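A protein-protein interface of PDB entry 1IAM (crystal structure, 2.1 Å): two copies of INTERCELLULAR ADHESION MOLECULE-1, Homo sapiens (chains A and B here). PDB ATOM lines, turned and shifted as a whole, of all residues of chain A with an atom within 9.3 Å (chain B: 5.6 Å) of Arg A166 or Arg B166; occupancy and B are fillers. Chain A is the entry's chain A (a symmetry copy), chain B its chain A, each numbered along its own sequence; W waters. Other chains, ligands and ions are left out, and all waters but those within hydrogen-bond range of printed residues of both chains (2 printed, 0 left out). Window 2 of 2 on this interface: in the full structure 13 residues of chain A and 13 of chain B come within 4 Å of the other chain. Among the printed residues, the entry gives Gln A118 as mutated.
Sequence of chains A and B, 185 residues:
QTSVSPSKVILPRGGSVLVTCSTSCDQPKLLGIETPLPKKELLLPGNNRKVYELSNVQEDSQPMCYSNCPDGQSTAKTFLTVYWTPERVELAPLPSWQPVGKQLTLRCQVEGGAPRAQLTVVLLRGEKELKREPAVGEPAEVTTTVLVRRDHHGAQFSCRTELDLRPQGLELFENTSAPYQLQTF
The side-chain carboxylate (OD2) of Asp A164 lies within salt-bridge range of the guanidinium group (NH2) of Arg A166 (2.9 Å). The backbone carbonyl oxygen (O) of Leu A165 lies close to the side-chain amide nitrogen (NE2) of Gln A168. O of Leu B165 lies close to NE2 of Gln B168, 3.3 Å away. The side-chain carboxylate of Asp B164 is in salt-bridge range of the guanidinium group of Arg B166 (2.9 Å).
Water W2 lies within hydrogen-bond range of the backbone carbonyl oxygen (O) of Gln B168 (2.7 Å) and the backbone carbonyl oxygen (O) of Gln A168 (2.7 Å). Water W1 lies within hydrogen-bond range of O of Arg B166 (3.1 Å) and O of Arg A166 (3.1 Å).
Arg A166 touches one residue of chain B. Printed residues of chain B within 4 Å of Gly A169: Pro B167 (3.7 Å), Gln B168 (3.7 Å) and Gly B169 (3.8 Å). Of chain A, only Arg A166 comes within 4 Å of Arg B166. Of chain A, only Gly A169 comes within 4 Å of Pro B167. Printed residues of chain A within 4 Å of Gln B168: Gly A169. The nearest residue of chain B that does not touch Arg A166 is Pro B167 (4.1 Å). The nearest printed residue of chain B that does not touch Pro A167 is Arg B166 (4.1 Å).
Among the printed residues, pairs that only touch across the chains: Gly A169 with Pro B167, Pro A167 with Gly B169, Gln A168 with Gly B169, Gly A169 with Gln B168, Gly A169 with Gly B169 and Arg A166 with Arg B166.
Of the 9 printed residues of chain B, 4 touch a printed residue of chain A. Printed residues of chain B that touch a printed residue of chain A: Arg B166, Pro B167, Gln B168 and Gly B169. Of the 17 printed residues of chain A, 4 touch a printed residue of chain B. Among the printed residues, no Asp or Glu carboxylate lies within 4 Å of a Lys or Arg side-chain nitrogen of the other chain.
Arg B166 touches its own counterpart, Arg A166. Pro A167 touches Gly B169, and with the chains exchanged Gly A169 touches Pro B167. Gln A168 touches Gly B169, and with the chains exchanged Gly A169 touches Gln B168. Gly A169 touches its own counterpart, Gly B169. Positions printed for both chains: 164, 165, 166, 167, 168, 169, 170, 171 and 172.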
ATOM      1  N   ILE A  10     -14.699  25.962 -18.183  1.00  0.00           N
ATOM      2  CA  ILE A  10     -14.796  24.505 -18.177  1.00  0.00           C
ATOM      3  C   ILE A  10     -15.912  24.159 -17.212  1.00  0.00           C
ATOM      4  O   ILE A  10     -15.919  24.620 -16.071  1.00  0.00           O
ATOM      5  CB  ILE A  10     -13.486  23.801 -17.763  1.00  0.00           C
ATOM      6  CG1 ILE A  10     -13.671  22.285 -17.884  1.00  0.00           C
ATOM      7  CG2 ILE A  10     -13.044  24.217 -16.329  1.00  0.00           C
ATOM      8  CD1 ILE A  10     -12.367  21.511 -17.953  1.00  0.00           C
ATOM      9  N   PRO A 115     -13.104  16.551 -21.526  1.00  0.00           N
ATOM     10  CA  PRO A 115     -12.448  16.718 -22.825  1.00  0.00           C
ATOM     11  C   PRO A 115     -11.446  15.595 -23.137  1.00  0.00           C
ATOM     12  O   PRO A 115     -10.664  15.193 -22.264  1.00  0.00           O
ATOM     13  CB  PRO A 115     -11.790  18.100 -22.697  1.00  0.00           C
ATOM     14  CG  PRO A 115     -11.463  18.199 -21.236  1.00  0.00           C
ATOM     15  CD  PRO A 115     -12.693  17.622 -20.587  1.00  0.00           C
ATOM     16  N   GLN A 118      -7.593  15.580 -22.448  1.00  0.00           N
ATOM     17  CA  GLN A 118      -7.023  15.406 -21.105  1.00  0.00           C
ATOM     18  C   GLN A 118      -7.351  14.029 -20.532  1.00  0.00           C
ATOM     19  O   GLN A 118      -7.156  13.787 -19.343  1.00  0.00           O
ATOM     20  CB  GLN A 118      -7.538  16.509 -20.172  1.00  0.00           C
ATOM     21  CG  GLN A 118      -7.109  17.930 -20.584  1.00  0.00           C
ATOM     22  CD  GLN A 118      -5.674  18.276 -20.183  1.00  0.00           C
ATOM     23  OE1 GLN A 118      -5.013  17.550 -19.418  1.00  0.00           O
ATOM     24  NE2 GLN A 118      -5.200  19.418 -20.661  1.00  0.00           N
ATOM     25  N   ARG A 132       0.171   3.298 -21.500  1.00  0.00           N
ATOM     26  CA  ARG A 132      -0.509   4.589 -21.270  1.00  0.00           C
ATOM     27  C   ARG A 132      -0.683   5.192 -22.648  1.00  0.00           C
ATOM     28  O   ARG A 132       0.265   5.162 -23.433  1.00  0.00           O
ATOM     29  CB  ARG A 132       0.352   5.565 -20.458  1.00  0.00           C
ATOM     30  CG  ARG A 132       0.367   5.309 -19.002  1.00  0.00           C
ATOM     31  CD  ARG A 132       1.105   6.405 -18.272  1.00  0.00           C
ATOM     32  NE  ARG A 132       0.341   7.644 -18.249  1.00  0.00           N
ATOM     33  CZ  ARG A 132      -0.548   7.975 -17.307  1.00  0.00           C
ATOM     34  NH1 ARG A 132      -0.801   7.167 -16.280  1.00  0.00           N
ATOM     35  NH2 ARG A 132      -1.185   9.129 -17.403  1.00  0.00           N
ATOM     36  N   GLU A 162      -7.786   8.341 -16.795  1.00  0.00           N
ATOM     37  CA  GLU A 162      -7.424   9.512 -15.993  1.00  0.00           C
ATOM     38  C   GLU A 162      -7.889  10.765 -16.733  1.00  0.00           C
ATOM     39  O   GLU A 162      -7.394  11.070 -17.816  1.00  0.00           O
ATOM     40  CB  GLU A 162      -5.905   9.567 -15.779  1.00  0.00           C
ATOM     41  CG  GLU A 162      -5.378   8.420 -14.906  1.00  0.00           C
ATOM     42  CD  GLU A 162      -3.860   8.234 -14.968  1.00  0.00           C
ATOM     43  OE1 GLU A 162      -3.136   9.099 -15.505  1.00  0.00           O
ATOM     44  OE2 GLU A 162      -3.384   7.191 -14.489  1.00  0.00           O
ATOM     45  N   LEU A 163      -8.877  11.452 -16.174  1.00  0.00           N
ATOM     46  CA  LEU A 163      -9.408  12.683 -16.778  1.00  0.00           C
ATOM     47  C   LEU A 163      -8.742  13.748 -15.959  1.00  0.00           C
ATOM     48  O   LEU A 163      -9.252  14.125 -14.890  1.00  0.00           O
ATOM     49  CB  LEU A 163     -10.919  12.772 -16.572  1.00  0.00           C
ATOM     50  CG  LEU A 163     -11.805  13.348 -17.677  1.00  0.00           C
ATOM     51  CD1 LEU A 163     -13.050  14.012 -17.039  1.00  0.00           C
ATOM     52  CD2 LEU A 163     -11.051  14.319 -18.569  1.00  0.00           C
ATOM     53  N   ASP A 164      -7.602  14.224 -16.442  1.00  0.00           N
ATOM     54  CA  ASP A 164      -6.837  15.197 -15.674  1.00  0.00           C
ATOM     55  C   ASP A 164      -7.211  16.647 -15.898  1.00  0.00           C
ATOM     56  O   ASP A 164      -6.689  17.294 -16.809  1.00  0.00           O
ATOM     57  CB  ASP A 164      -5.340  14.999 -15.918  1.00  0.00           C
ATOM     58  CG  ASP A 164      -4.480  15.731 -14.899  1.00  0.00           C
ATOM     59  OD1 ASP A 164      -5.037  16.460 -14.037  1.00  0.00           O
ATOM     60  OD2 ASP A 164      -3.243  15.531 -14.929  1.00  0.00           O
ATOM     61  N   LEU A 165      -8.070  17.175 -15.032  1.00  0.00           N
ATOM     62  CA  LEU A 165      -8.504  18.569 -15.163  1.00  0.00           C
ATOM     63  C   LEU A 165      -7.760  19.512 -14.236  1.00  0.00           C
ATOM     64  O   LEU A 165      -8.144  20.682 -14.112  1.00  0.00           O
ATOM     65  CB  LEU A 165     -10.003  18.704 -14.885  1.00  0.00           C
ATOM     66  CG  LEU A 165     -10.987  18.435 -16.016  1.00  0.00           C
ATOM     67  CD1 LEU A 165     -10.356  17.784 -17.223  1.00  0.00           C
ATOM     68  CD2 LEU A 165     -12.127  17.638 -15.439  1.00  0.00           C
ATOM     69  N   ARG A 166      -6.732  19.009 -13.555  1.00  0.00           N
ATOM     70  CA  ARG A 166      -5.946  19.848 -12.651  1.00  0.00           C
ATOM     71  C   ARG A 166      -5.413  21.082 -13.367  1.00  0.00           C
ATOM     72  O   ARG A 166      -5.391  22.162 -12.794  1.00  0.00           O
ATOM     73  CB  ARG A 166      -4.786  19.055 -12.034  1.00  0.00           C
ATOM     74  CG  ARG A 166      -5.230  18.076 -10.964  1.00  0.00           C
ATOM     75  CD  ARG A 166      -4.104  17.192 -10.478  1.00  0.00           C
ATOM     76  NE  ARG A 166      -3.589  16.299 -11.517  1.00  0.00           N
ATOM     77  CZ  ARG A 166      -2.524  15.503 -11.368  1.00  0.00           C
ATOM     78  NH1 ARG A 166      -1.864  15.488 -10.227  1.00  0.00           N
ATOM     79  NH2 ARG A 166      -2.107  14.742 -12.372  1.00  0.00           N
ATOM     80  N   PRO A 167      -4.941  20.945 -14.623  1.00  0.00           N
ATOM     81  CA  PRO A 167      -4.455  22.189 -15.228  1.00  0.00           C
ATOM     82  C   PRO A 167      -5.547  23.230 -15.512  1.00  0.00           C
ATOM     83  O   PRO A 167      -5.238  24.354 -15.894  1.00  0.00           O
ATOM     84  CB  PRO A 167      -3.747  21.717 -16.496  1.00  0.00           C
ATOM     85  CG  PRO A 167      -4.351  20.390 -16.785  1.00  0.00           C
ATOM     86  CD  PRO A 167      -4.538  19.779 -15.430  1.00  0.00           C
ATOM     87  N   GLN A 168      -6.808  22.848 -15.306  1.00  0.00           N
ATOM     88  CA  GLN A 168      -7.941  23.740 -15.526  1.00  0.00           C
ATOM     89  C   GLN A 168      -8.448  24.257 -14.186  1.00  0.00           C
ATOM     90  O   GLN A 168      -9.396  25.031 -14.140  1.00  0.00           O
ATOM     91  CB  GLN A 168      -9.083  23.014 -16.247  1.00  0.00           C
ATOM     92  CG  GLN A 168      -8.951  22.898 -17.775  1.00  0.00           C
ATOM     93  CD  GLN A 168      -7.912  21.894 -18.237  1.00  0.00           C
ATOM     94  OE1 GLN A 168      -7.495  21.916 -19.409  1.00  0.00           O
ATOM     95  NE2 GLN A 168      -7.485  21.007 -17.339  1.00  0.00           N
ATOM     96  N   GLY A 169      -7.849  23.787 -13.096  1.00  0.00           N
ATOM     97  CA  GLY A 169      -8.251  24.232 -11.781  1.00  0.00           C
ATOM     98  C   GLY A 169      -9.111  23.246 -11.020  1.00  0.00           C
ATOM     99  O   GLY A 169      -9.606  23.564  -9.947  1.00  0.00           O
ATOM    100  N   LEU A 170      -9.304  22.050 -11.577  1.00  0.00           N
ATOM    101  CA  LEU A 170     -10.123  21.043 -10.904  1.00  0.00           C
ATOM    102  C   LEU A 170      -9.240  19.903 -10.407  1.00  0.00           C
ATOM    103  O   LEU A 170      -8.137  20.136  -9.913  1.00  0.00           O
ATOM    104  CB  LEU A 170     -11.226  20.524 -11.837  1.00  0.00           C
ATOM    105  CG  LEU A 170     -12.177  21.558 -12.454  1.00  0.00           C
ATOM    106  CD1 LEU A 170     -13.199  20.845 -13.314  1.00  0.00           C
ATOM    107  CD2 LEU A 170     -12.882  22.354 -11.366  1.00  0.00           C
ATOM    108  N   GLU A 171      -9.705  18.672 -10.538  1.00  0.00           N
ATOM    109  CA  GLU A 171      -8.912  17.556 -10.084  1.00  0.00           C
ATOM    110  C   GLU A 171      -8.833  16.474 -11.140  1.00  0.00           C
ATOM    111  O   GLU A 171      -9.306  16.642 -12.268  1.00  0.00           O
ATOM    112  CB  GLU A 171      -9.457  17.010  -8.762  1.00  0.00           C
ATOM    113  CG  GLU A 171     -10.894  16.513  -8.793  1.00  0.00           C
ATOM    114  CD  GLU A 171     -11.465  16.341  -7.392  1.00  0.00           C
ATOM    115  OE1 GLU A 171     -11.392  17.320  -6.616  1.00  0.00           O
ATOM    116  OE2 GLU A 171     -11.977  15.240  -7.056  1.00  0.00           O
ATOM    117  N   LEU A 172      -8.107  15.422 -10.809  1.00  0.00           N
ATOM    118  CA  LEU A 172      -7.959  14.286 -11.697  1.00  0.00           C
ATOM    119  C   LEU A 172      -9.072  13.354 -11.282  1.00  0.00           C
ATOM    120  O   LEU A 172      -9.208  13.061 -10.104  1.00  0.00           O
ATOM    121  CB  LEU A 172      -6.626  13.596 -11.427  1.00  0.00           C
ATOM    122  CG  LEU A 172      -6.471  12.161 -11.921  1.00  0.00           C
ATOM    123  CD1 LEU A 172      -6.202  12.187 -13.397  1.00  0.00           C
ATOM    124  CD2 LEU A 172      -5.310  11.501 -11.180  1.00  0.00           C
ATOM    125  N   PHE A 173      -9.888  12.935 -12.238  1.00  0.00           N
ATOM    126  CA  PHE A 173     -10.975  12.011 -11.971  1.00  0.00           C
ATOM    127  C   PHE A 173     -10.568  10.663 -12.575  1.00  0.00           C
ATOM    128  O   PHE A 173     -10.281  10.576 -13.773  1.00  0.00           O
ATOM    129  CB  PHE A 173     -12.261  12.535 -12.631  1.00  0.00           C
ATOM    130  CG  PHE A 173     -12.694  13.889 -12.129  1.00  0.00           C
ATOM    131  CD1 PHE A 173     -13.335  14.013 -10.909  1.00  0.00           C
ATOM    132  CD2 PHE A 173     -12.423  15.035 -12.859  1.00  0.00           C
ATOM    133  CE1 PHE A 173     -13.694  15.263 -10.420  1.00  0.00           C
ATOM    134  CE2 PHE A 173     -12.777  16.297 -12.380  1.00  0.00           C
ATOM    135  CZ  PHE A 173     -13.414  16.409 -11.155  1.00  0.00           C
ATOM    136  N   GLU A 174     -10.538   9.613 -11.764  1.00  0.00           N
ATOM    137  CA  GLU A 174     -10.157   8.284 -12.255  1.00  0.00           C
ATOM    138  C   GLU A 174     -11.341   7.308 -12.291  1.00  0.00           C
ATOM    139  O   GLU A 174     -12.269   7.409 -11.495  1.00  0.00           O
ATOM    140  CB  GLU A 174      -9.127   7.622 -11.334  1.00  0.00           C
ATOM    141  CG  GLU A 174      -8.043   8.475 -10.718  1.00  0.00           C
ATOM    142  CD  GLU A 174      -7.199   7.638  -9.750  1.00  0.00           C
ATOM    143  OE1 GLU A 174      -6.386   6.807 -10.228  1.00  0.00           O
ATOM    144  OE2 GLU A 174      -7.399   7.735  -8.513  1.00  0.00           O
ATOM    145  N   ASP B 164       2.790  30.914  -8.562  1.00  0.00           N
ATOM    146  CA  ASP B 164       2.273  29.780  -9.317  1.00  0.00           C
ATOM    147  C   ASP B 164       0.783  29.539  -9.195  1.00  0.00           C
ATOM    148  O   ASP B 164       0.335  28.844  -8.280  1.00  0.00           O
ATOM    149  CB  ASP B 164       3.041  28.509  -8.948  1.00  0.00           C
ATOM    150  CG  ASP B 164       2.801  27.376  -9.933  1.00  0.00           C
ATOM    151  OD1 ASP B 164       1.977  27.542 -10.871  1.00  0.00           O
ATOM    152  OD2 ASP B 164       3.481  26.332  -9.799  1.00  0.00           O
ATOM    153  N   LEU B 165       0.022  30.063 -10.150  1.00  0.00           N
ATOM    154  CA  LEU B 165      -1.434  29.894 -10.122  1.00  0.00           C
ATOM    155  C   LEU B 165      -1.921  28.785 -11.035  1.00  0.00           C
ATOM    156  O   LEU B 165      -3.133  28.650 -11.246  1.00  0.00           O
ATOM    157  CB  LEU B 165      -2.143  31.191 -10.521  1.00  0.00           C
ATOM    158  CG  LEU B 165      -2.383  32.255  -9.457  1.00  0.00           C
ATOM    159  CD1 LEU B 165      -1.627  32.006  -8.174  1.00  0.00           C
ATOM    160  CD2 LEU B 165      -2.074  33.590 -10.080  1.00  0.00           C
ATOM    161  N   ARG B 166      -0.995  28.020 -11.609  1.00  0.00           N
ATOM    162  CA  ARG B 166      -1.372  26.915 -12.491  1.00  0.00           C
ATOM    163  C   ARG B 166      -2.335  25.961 -11.798  1.00  0.00           C
ATOM    164  O   ARG B 166      -3.266  25.471 -12.421  1.00  0.00           O
ATOM    165  CB  ARG B 166      -0.131  26.152 -12.976  1.00  0.00           C
ATOM    166  CG  ARG B 166       0.663  26.903 -14.027  1.00  0.00           C
ATOM    167  CD  ARG B 166       1.962  26.215 -14.380  1.00  0.00           C
ATOM    168  NE  ARG B 166       2.904  26.163 -13.261  1.00  0.00           N
ATOM    169  CZ  ARG B 166       4.072  25.511 -13.287  1.00  0.00           C
ATOM    170  NH1 ARG B 166       4.441  24.858 -14.372  1.00  0.00           N
ATOM    171  NH2 ARG B 166       4.856  25.492 -12.218  1.00  0.00           N
ATOM    172  N   PRO B 167      -2.116  25.649 -10.504  1.00  0.00           N
ATOM    173  CA  PRO B 167      -3.099  24.728  -9.927  1.00  0.00           C
ATOM    174  C   PRO B 167      -4.512  25.311  -9.779  1.00  0.00           C
ATOM    175  O   PRO B 167      -5.440  24.589  -9.431  1.00  0.00           O
ATOM    176  CB  PRO B 167      -2.480  24.339  -8.585  1.00  0.00           C
ATOM    177  CG  PRO B 167      -1.537  25.447  -8.278  1.00  0.00           C
ATOM    178  CD  PRO B 167      -0.953  25.799  -9.611  1.00  0.00           C
ATOM    179  N   GLN B 168      -4.657  26.606 -10.063  1.00  0.00           N
ATOM    180  CA  GLN B 168      -5.946  27.285  -9.976  1.00  0.00           C
ATOM    181  C   GLN B 168      -6.519  27.468 -11.375  1.00  0.00           C
ATOM    182  O   GLN B 168      -7.605  28.013 -11.532  1.00  0.00           O
ATOM    183  CB  GLN B 168      -5.803  28.658  -9.309  1.00  0.00           C
ATOM    184  CG  GLN B 168      -5.761  28.662  -7.772  1.00  0.00           C
ATOM    185  CD  GLN B 168      -4.462  28.148  -7.181  1.00  0.00           C
ATOM    186  OE1 GLN B 168      -4.403  27.818  -5.984  1.00  0.00           O
ATOM    187  NE2 GLN B 168      -3.411  28.078  -7.999  1.00  0.00           N
ATOM    188  N   GLY B 169      -5.765  27.060 -12.391  1.00  0.00           N
ATOM    189  CA  GLY B 169      -6.232  27.179 -13.753  1.00  0.00           C
ATOM    190  C   GLY B 169      -5.622  28.328 -14.528  1.00  0.00           C
ATOM    191  O   GLY B 169      -6.031  28.595 -15.650  1.00  0.00           O
ATOM    192  N   LEU B 170      -4.654  29.020 -13.928  1.00  0.00           N
ATOM    193  CA  LEU B 170      -4.017  30.145 -14.612  1.00  0.00           C
ATOM    194  C   LEU B 170      -2.582  29.781 -14.981  1.00  0.00           C
ATOM    195  O   LEU B 170      -2.309  28.657 -15.400  1.00  0.00           O
ATOM    196  CB  LEU B 170      -4.062  31.409 -13.742  1.00  0.00           C
ATOM    197  CG  LEU B 170      -5.436  31.883 -13.252  1.00  0.00           C
ATOM    198  CD1 LEU B 170      -5.267  33.149 -12.438  1.00  0.00           C
ATOM    199  CD2 LEU B 170      -6.363  32.146 -14.429  1.00  0.00           C
ATOM    200  N   GLU B 171      -1.658  30.715 -14.825  1.00  0.00           N
ATOM    201  CA  GLU B 171      -0.285  30.427 -15.160  1.00  0.00           C
ATOM    202  C   GLU B 171       0.651  30.850 -14.049  1.00  0.00           C
ATOM    203  O   GLU B 171       0.220  31.269 -12.970  1.00  0.00           O
ATOM    204  CB  GLU B 171       0.093  31.081 -16.492  1.00  0.00           C
ATOM    205  CG  GLU B 171      -0.038  32.595 -16.547  1.00  0.00           C
ATOM    206  CD  GLU B 171      -0.005  33.116 -17.977  1.00  0.00           C
ATOM    207  OE1 GLU B 171      -0.807  32.610 -18.794  1.00  0.00           O
ATOM    208  OE2 GLU B 171       0.817  34.016 -18.296  1.00  0.00           O
ATOM    209  N   LEU B 172       1.929  30.602 -14.270  1.00  0.00           N
ATOM    210  CA  LEU B 172       2.956  30.977 -13.317  1.00  0.00           C
ATOM    211  C   LEU B 172       3.386  32.351 -13.770  1.00  0.00           C
ATOM    212  O   LEU B 172       3.689  32.536 -14.939  1.00  0.00           O
ATOM    213  CB  LEU B 172       4.144  30.031 -13.449  1.00  0.00           C
ATOM    214  CG  LEU B 172       5.477  30.501 -12.874  1.00  0.00           C
ATOM    215  CD1 LEU B 172       5.448  30.319 -11.385  1.00  0.00           C
ATOM    216  CD2 LEU B 172       6.605  29.676 -13.489  1.00  0.00           C
HETATM  217  O   HOH W   1      -2.350  22.533 -12.499  1.00  0.00           O
HETATM  218  O   HOH W   2      -9.882  27.418 -12.912  1.00  0.00           O
